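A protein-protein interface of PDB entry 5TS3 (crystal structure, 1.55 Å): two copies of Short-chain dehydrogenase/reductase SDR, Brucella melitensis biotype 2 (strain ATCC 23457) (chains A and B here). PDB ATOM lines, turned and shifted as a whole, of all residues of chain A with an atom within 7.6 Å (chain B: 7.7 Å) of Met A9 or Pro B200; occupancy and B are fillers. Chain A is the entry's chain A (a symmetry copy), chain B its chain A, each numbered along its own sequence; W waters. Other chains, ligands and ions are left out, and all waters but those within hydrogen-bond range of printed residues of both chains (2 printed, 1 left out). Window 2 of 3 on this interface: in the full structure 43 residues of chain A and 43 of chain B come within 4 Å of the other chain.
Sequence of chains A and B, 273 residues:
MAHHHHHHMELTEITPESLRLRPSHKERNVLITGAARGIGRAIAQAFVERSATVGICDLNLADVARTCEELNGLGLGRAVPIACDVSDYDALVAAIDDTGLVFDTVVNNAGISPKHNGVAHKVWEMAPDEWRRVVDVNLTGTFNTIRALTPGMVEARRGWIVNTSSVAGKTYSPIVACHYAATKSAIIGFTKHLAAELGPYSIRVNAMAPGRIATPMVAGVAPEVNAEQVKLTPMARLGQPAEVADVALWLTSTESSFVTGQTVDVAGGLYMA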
ATOM      1  N   MET A   9     -22.924  14.463   6.808  1.00  0.00           N
ATOM      2  CA  MET A   9     -22.548  15.040   5.520  1.00  0.00           C
ATOM      3  C   MET A   9     -23.509  14.620   4.412  1.00  0.00           C
ATOM      4  O   MET A   9     -23.640  13.432   4.114  1.00  0.00           O
ATOM      5  CB  MET A   9     -21.123  14.633   5.150  1.00  0.00           C
ATOM      6  CG  MET A   9     -20.748  14.959   3.716  1.00  0.00           C
ATOM      7  SD  MET A   9     -20.562  16.729   3.412  1.00  0.00           S
ATOM      8  CE  MET A   9     -19.071  17.080   4.345  1.00  0.00           C
ATOM      9  N   GLU A  10     -24.164  15.598   3.793  1.00  0.00           N
ATOM     10  CA  GLU A  10     -25.176  15.329   2.782  1.00  0.00           C
ATOM     11  C   GLU A  10     -24.564  15.287   1.382  1.00  0.00           C
ATOM     12  O   GLU A  10     -23.416  15.678   1.156  1.00  0.00           O
ATOM     13  CB  GLU A  10     -26.281  16.384   2.843  1.00  0.00           C
ATOM     14  N   LEU A  11     -25.357  14.797   0.430  1.00  0.00           N
ATOM     15  CA  LEU A  11     -24.946  14.812  -0.967  1.00  0.00           C
ATOM     16  C   LEU A  11     -24.947  16.236  -1.505  1.00  0.00           C
ATOM     17  O   LEU A  11     -25.853  17.027  -1.225  1.00  0.00           O
ATOM     18  CB  LEU A  11     -25.868  13.932  -1.810  1.00  0.00           C
ATOM     19  CG  LEU A  11     -25.830  12.431  -1.523  1.00  0.00           C
ATOM     20  CD1 LEU A  11     -26.769  11.682  -2.458  1.00  0.00           C
ATOM     21  CD2 LEU A  11     -24.415  11.911  -1.665  1.00  0.00           C
ATOM     22  N   THR A  12     -23.919  16.559  -2.286  1.00  0.00           N
ATOM     23  CA  THR A  12     -23.701  17.902  -2.802  1.00  0.00           C
ATOM     24  C   THR A  12     -23.826  18.010  -4.316  1.00  0.00           C
ATOM     25  O   THR A  12     -24.195  19.073  -4.818  1.00  0.00           O
ATOM     26  CB  THR A  12     -22.307  18.406  -2.383  1.00  0.00           C
ATOM     27  OG1 THR A  12     -21.370  17.314  -2.411  1.00  0.00           O
ATOM     28  CG2 THR A  12     -22.350  18.995  -0.984  1.00  0.00           C
ATOM     29  N   VAL A 230     -15.857   6.238   8.410  1.00  0.00           N
ATOM     30  CA  VAL A 230     -16.347   7.527   7.931  1.00  0.00           C
ATOM     31  C   VAL A 230     -15.414   8.645   8.385  1.00  0.00           C
ATOM     32  O   VAL A 230     -15.112   9.569   7.615  1.00  0.00           O
ATOM     33  CB  VAL A 230     -17.800   7.751   8.388  1.00  0.00           C
ATOM     34  CG1 VAL A 230     -18.223   9.189   8.143  1.00  0.00           C
ATOM     35  CG2 VAL A 230     -18.728   6.802   7.635  1.00  0.00           C
ATOM     36  N   THR A 233     -12.615   8.972   6.130  1.00  0.00           N
ATOM     37  CA  THR A 233     -12.979   9.353   4.771  1.00  0.00           C
ATOM     38  C   THR A 233     -12.986  10.870   4.669  1.00  0.00           C
ATOM     39  O   THR A 233     -13.812  11.518   5.332  1.00  0.00           O
ATOM     40  CB  THR A 233     -14.359   8.797   4.413  1.00  0.00           C
ATOM     41  OG1 THR A 233     -14.362   7.371   4.578  1.00  0.00           O
ATOM     42  CG2 THR A 233     -14.720   9.140   2.971  1.00  0.00           C
ATOM     43  N   PRO A 234     -12.089  11.479   3.882  1.00  0.00           N
ATOM     44  CA  PRO A 234     -12.089  12.947   3.744  1.00  0.00           C
ATOM     45  C   PRO A 234     -13.452  13.534   3.416  1.00  0.00           C
ATOM     46  O   PRO A 234     -13.838  14.534   4.029  1.00  0.00           O
ATOM     47  CB  PRO A 234     -11.073  13.178   2.615  1.00  0.00           C
ATOM     48  CG  PRO A 234     -10.080  12.043   2.779  1.00  0.00           C
ATOM     49  CD  PRO A 234     -10.962  10.855   3.167  1.00  0.00           C
ATOM     50  N   MET A 235     -14.212  12.925   2.499  1.00  0.00           N
ATOM     51  CA  MET A 235     -15.518  13.476   2.142  1.00  0.00           C
ATOM     52  C   MET A 235     -16.596  13.187   3.184  1.00  0.00           C
ATOM     53  O   MET A 235     -17.735  13.631   3.011  1.00  0.00           O
ATOM     54  CB  MET A 235     -15.930  12.974   0.754  1.00  0.00           C
ATOM     55  CG  MET A 235     -14.987  13.544  -0.320  1.00  0.00           C
ATOM     56  SD  MET A 235     -15.459  13.174  -2.021  1.00  0.00           S
ATOM     57  CE  MET A 235     -17.028  14.053  -2.123  1.00  0.00           C
ATOM     58  N   ALA A 236     -16.260  12.465   4.256  1.00  0.00           N
ATOM     59  CA  ALA A 236     -17.028  12.462   5.504  1.00  0.00           C
ATOM     60  C   ALA A 236     -18.375  11.755   5.374  1.00  0.00           C
ATOM     61  O   ALA A 236     -19.322  12.081   6.097  1.00  0.00           O
ATOM     62  CB  ALA A 236     -17.230  13.890   6.028  1.00  0.00           C
ATOM     63  N   ARG A 237     -18.461  10.763   4.490  1.00  0.00           N
ATOM     64  CA  ARG A 237     -19.686   9.990   4.327  1.00  0.00           C
ATOM     65  C   ARG A 237     -19.352   8.683   3.630  1.00  0.00           C
ATOM     66  O   ARG A 237     -18.275   8.532   3.046  1.00  0.00           O
ATOM     67  CB  ARG A 237     -20.731  10.758   3.519  1.00  0.00           C
ATOM     68  CG  ARG A 237     -20.272  11.105   2.102  1.00  0.00           C
ATOM     69  CD  ARG A 237     -21.395  11.766   1.330  1.00  0.00           C
ATOM     70  NE  ARG A 237     -21.010  12.208  -0.008  1.00  0.00           N
ATOM     71  CZ  ARG A 237     -21.050  11.435  -1.093  1.00  0.00           C
ATOM     72  NH1 ARG A 237     -21.443  10.166  -1.002  1.00  0.00           N
ATOM     73  NH2 ARG A 237     -20.708  11.932  -2.278  1.00  0.00           N
ATOM     74  N   LEU A 238     -20.290   7.738   3.712  1.00  0.00           N
ATOM     75  CA  LEU A 238     -20.252   6.567   2.845  1.00  0.00           C
ATOM     76  C   LEU A 238     -20.579   6.975   1.418  1.00  0.00           C
ATOM     77  O   LEU A 238     -21.306   7.941   1.183  1.00  0.00           O
ATOM     78  CB  LEU A 238     -21.260   5.515   3.310  1.00  0.00           C
ATOM     79  CG  LEU A 238     -21.075   4.948   4.712  1.00  0.00           C
ATOM     80  CD1 LEU A 238     -22.258   4.053   5.094  1.00  0.00           C
ATOM     81  CD2 LEU A 238     -19.765   4.183   4.770  1.00  0.00           C
ATOM     82  N   GLY A 268     -14.131   8.565  -1.979  1.00  0.00           N
ATOM     83  CA  GLY A 268     -14.196   9.800  -1.220  1.00  0.00           C
ATOM     84  C   GLY A 268     -12.928  10.149  -0.469  1.00  0.00           C
ATOM     85  O   GLY A 268     -12.982  10.907   0.508  1.00  0.00           O
ATOM     86  N   VAL B 154     -13.289  26.529  -0.205  1.00  0.00           N
ATOM     87  CA  VAL B 154     -13.521  26.043   1.152  1.00  0.00           C
ATOM     88  C   VAL B 154     -14.671  26.802   1.800  1.00  0.00           C
ATOM     89  O   VAL B 154     -15.539  26.210   2.450  1.00  0.00           O
ATOM     90  CB  VAL B 154     -12.222  26.145   1.975  1.00  0.00           C
ATOM     91  CG1 VAL B 154     -12.506  25.939   3.464  1.00  0.00           C
ATOM     92  CG2 VAL B 154     -11.214  25.118   1.464  1.00  0.00           C
ATOM     93  N   ARG B 157     -17.850  25.593   0.371  1.00  0.00           N
ATOM     94  CA  ARG B 157     -17.957  24.136   0.414  1.00  0.00           C
ATOM     95  C   ARG B 157     -18.313  23.593  -0.967  1.00  0.00           C
ATOM     96  O   ARG B 157     -19.216  22.767  -1.133  1.00  0.00           O
ATOM     97  CB  ARG B 157     -18.963  23.685   1.475  1.00  0.00           C
ATOM     98  CG  ARG B 157     -18.484  23.962   2.890  1.00  0.00           C
ATOM     99  CD  ARG B 157     -19.468  23.451   3.929  1.00  0.00           C
ATOM    100  NE  ARG B 157     -18.835  23.333   5.242  1.00  0.00           N
ATOM    101  CZ  ARG B 157     -18.184  22.251   5.660  1.00  0.00           C
ATOM    102  NH1 ARG B 157     -18.082  21.190   4.869  1.00  0.00           N
ATOM    103  NH2 ARG B 157     -17.633  22.228   6.865  1.00  0.00           N
ATOM    104  N   LEU B 194      -4.018  16.799  -1.455  1.00  0.00           N
ATOM    105  CA  LEU B 194      -5.042  17.830  -1.602  1.00  0.00           C
ATOM    106  C   LEU B 194      -6.444  17.254  -1.441  1.00  0.00           C
ATOM    107  O   LEU B 194      -7.310  17.877  -0.813  1.00  0.00           O
ATOM    108  CB  LEU B 194      -4.901  18.499  -2.967  1.00  0.00           C
ATOM    109  CG  LEU B 194      -3.645  19.343  -3.213  1.00  0.00           C
ATOM    110  CD1 LEU B 194      -3.507  19.601  -4.708  1.00  0.00           C
ATOM    111  CD2 LEU B 194      -3.763  20.654  -2.452  1.00  0.00           C
ATOM    112  N   ALA B 195      -6.701  16.080  -2.028  1.00  0.00           N
ATOM    113  CA  ALA B 195      -8.022  15.474  -1.898  1.00  0.00           C
ATOM    114  C   ALA B 195      -8.374  15.256  -0.434  1.00  0.00           C
ATOM    115  O   ALA B 195      -9.528  15.437  -0.026  1.00  0.00           O
ATOM    116  CB  ALA B 195      -8.065  14.150  -2.660  1.00  0.00           C
ATOM    117  N   ALA B 196      -7.386  14.886   0.379  1.00  0.00           N
ATOM    118  CA  ALA B 196      -7.671  14.638   1.784  1.00  0.00           C
ATOM    119  C   ALA B 196      -7.911  15.940   2.535  1.00  0.00           C
ATOM    120  O   ALA B 196      -8.783  15.998   3.409  1.00  0.00           O
ATOM    121  CB  ALA B 196      -6.528  13.855   2.412  1.00  0.00           C
ATOM    122  N   GLU B 197      -7.144  16.994   2.217  1.00  0.00           N
ATOM    123  CA  GLU B 197      -7.337  18.263   2.919  1.00  0.00           C
ATOM    124  C   GLU B 197      -8.657  18.912   2.547  1.00  0.00           C
ATOM    125  O   GLU B 197      -9.288  19.559   3.393  1.00  0.00           O
ATOM    126  CB  GLU B 197      -6.209  19.254   2.625  1.00  0.00           C
ATOM    127  CG  GLU B 197      -4.888  18.906   3.271  1.00  0.00           C
ATOM    128  CD  GLU B 197      -3.860  20.015   3.107  1.00  0.00           C
ATOM    129  OE1 GLU B 197      -4.122  20.977   2.357  1.00  0.00           O
ATOM    130  OE2 GLU B 197      -2.791  19.935   3.745  1.00  0.00           O
ATOM    131  N   LEU B 198      -9.072  18.783   1.286  1.00  0.00           N
ATOM    132  CA  LEU B 198     -10.211  19.539   0.778  1.00  0.00           C
ATOM    133  C   LEU B 198     -11.510  18.751   0.807  1.00  0.00           C
ATOM    134  O   LEU B 198     -12.585  19.362   0.798  1.00  0.00           O
ATOM    135  CB  LEU B 198      -9.920  20.037  -0.651  1.00  0.00           C
ATOM    136  CG  LEU B 198      -8.745  21.025  -0.737  1.00  0.00           C
ATOM    137  CD1 LEU B 198      -8.229  21.135  -2.173  1.00  0.00           C
ATOM    138  CD2 LEU B 198      -9.139  22.412  -0.234  1.00  0.00           C
ATOM    139  N   GLY B 199     -11.428  17.416   0.873  1.00  0.00           N
ATOM    140  CA  GLY B 199     -12.616  16.590   0.966  1.00  0.00           C
ATOM    141  C   GLY B 199     -13.618  16.958   2.041  1.00  0.00           C
ATOM    142  O   GLY B 199     -14.831  16.840   1.806  1.00  0.00           O
ATOM    143  N   PRO B 200     -13.177  17.357   3.242  1.00  0.00           N
ATOM    144  CA  PRO B 200     -14.154  17.707   4.291  1.00  0.00           C
ATOM    145  C   PRO B 200     -15.078  18.839   3.898  1.00  0.00           C
ATOM    146  O   PRO B 200     -16.151  18.996   4.507  1.00  0.00           O
ATOM    147  CB  PRO B 200     -13.266  18.100   5.477  1.00  0.00           C
ATOM    148  CG  PRO B 200     -12.012  17.302   5.267  1.00  0.00           C
ATOM    149  CD  PRO B 200     -11.800  17.341   3.781  1.00  0.00           C
ATOM    150  N   TYR B 201     -14.690  19.638   2.907  1.00  0.00           N
ATOM    151  CA  TYR B 201     -15.483  20.740   2.393  1.00  0.00           C
ATOM    152  C   TYR B 201     -16.167  20.369   1.086  1.00  0.00           C
ATOM    153  O   TYR B 201     -16.620  21.259   0.358  1.00  0.00           O
ATOM    154  CB  TYR B 201     -14.595  21.980   2.242  1.00  0.00           C
ATOM    155  CG  TYR B 201     -13.866  22.239   3.537  1.00  0.00           C
ATOM    156  CD1 TYR B 201     -14.513  22.867   4.587  1.00  0.00           C
ATOM    157  CD2 TYR B 201     -12.555  21.794   3.737  1.00  0.00           C
ATOM    158  CE1 TYR B 201     -13.884  23.069   5.801  1.00  0.00           C
ATOM    159  CE2 TYR B 201     -11.919  21.986   4.950  1.00  0.00           C
ATOM    160  CZ  TYR B 201     -12.593  22.630   5.972  1.00  0.00           C
ATOM    161  OH  TYR B 201     -11.990  22.833   7.187  1.00  0.00           O
ATOM    162  N   SER B 202     -16.212  19.061   0.776  1.00  0.00           N
ATOM    163  CA  SER B 202     -16.876  18.489  -0.391  1.00  0.00           C
ATOM    164  C   SER B 202     -16.201  18.859  -1.708  1.00  0.00           C
ATOM    165  O   SER B 202     -16.815  18.745  -2.771  1.00  0.00           O
ATOM    166  CB  SER B 202     -18.362  18.872  -0.426  1.00  0.00           C
ATOM    167  OG  SER B 202     -18.980  18.533   0.808  1.00  0.00           O
ATOM    168  N   ILE B 203     -14.952  19.286  -1.656  1.00  0.00           N
ATOM    169  CA  ILE B 203     -14.171  19.637  -2.838  1.00  0.00           C
ATOM    170  C   ILE B 203     -13.421  18.397  -3.300  1.00  0.00           C
ATOM    171  O   ILE B 203     -12.769  17.728  -2.491  1.00  0.00           O
ATOM    172  CB  ILE B 203     -13.183  20.770  -2.511  1.00  0.00           C
ATOM    173  CG1 ILE B 203     -13.921  22.061  -2.120  1.00  0.00           C
ATOM    174  CG2 ILE B 203     -12.205  20.999  -3.674  1.00  0.00           C
ATOM    175  CD1 ILE B 203     -13.072  22.960  -1.242  1.00  0.00           C
HETATM  176  O   HOH W   1     -18.872  17.061  -3.675  1.00  0.00           O
HETATM  177  O   HOH W   2     -18.416  15.637   0.972  1.00  0.00           O
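OG of Ser B202 is in hydrogen-bond range of SD of Met A9 (3.5 Å).
The backbone carbonyl oxygen (O) of Pro A234 lies close to the backbone carbonyl oxygen (O) of Gly B199, at 3.4 Å.
The backbone carbonyl oxygen of Pro A234 lies close to the backbone nitrogen of Pro B200 (3.0 Å).
O of Pro B200 lies within hydrogen-bond range of NH1 of Arg B157, 2.9 Å away.
O of Gly A268 lies within hydrogen-bond range of N of Met A235, at 3.1 Å.
Met A9 touches Pro B200.
Thr A12 touches Ser B202.
Pro A234 touches Ala B195 (CB to O, 3.8 Å).
Ala B196 touches Pro A234.
Met A235 touches Gly B199.
Printed residues of chain B within 4 Å of Met A9: Pro B200 (3.5 Å) and Ser B202 (3.5 Å).
Of chain A, only Met A9 and Pro A234 come within 4 Å of Pro B200.
No residue of chain B comes within 4 Å of Glu A10.
Gly B199 touches just these residues of chain A: Pro A234 (3.1 Å) and Met A235 (3.4 Å).
Printed residues of chain A within 4 Å of Ala B195: Pro A234.
Of the printed residues of chain B, Thr A12 touches Ser B202 (3.8 Å).
Leu B198 touches none of the printed residues of chain A.
Leu A238 touches none of the printed residues of chain B.
The nearest residue of chain A that does not touch Pro B200 is Met A235 (4.6 Å).
The nearest printed residue of chain A that does not touch Ala B195 is Gly A268 (5.7 Å).
Of the 12 printed residues of chain B, 5 touch a printed residue of chain A.
Printed residues of chain A that touch a printed residue of chain B: Met A9, Thr A12, Pro A234 and Met A235.
Hydrophobic or aromatic side chains of chain A that line the printed part of chain B: Met A9, Pro A234 and Met A235.
Along chain A the printed residues that touch a printed residue of chain B span positions 9 to 235.
Among the printed residues, 8 pairs touch across the chains.
No position is printed for both chains.
Water W1 lies within hydrogen-bond range of O of Ser B202 (2.8 Å) and OG1 of Thr A12 (2.8 Å).
Water W2 lies within hydrogen-bond range of the backbone carbonyl oxygen (O) of Met A235 (2.9 Å), the side-chain hydroxyl (OG) of Ser B202 (3.0 Å) and the side-chain sulfur (SD) of Met A9 (3.4 Å).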
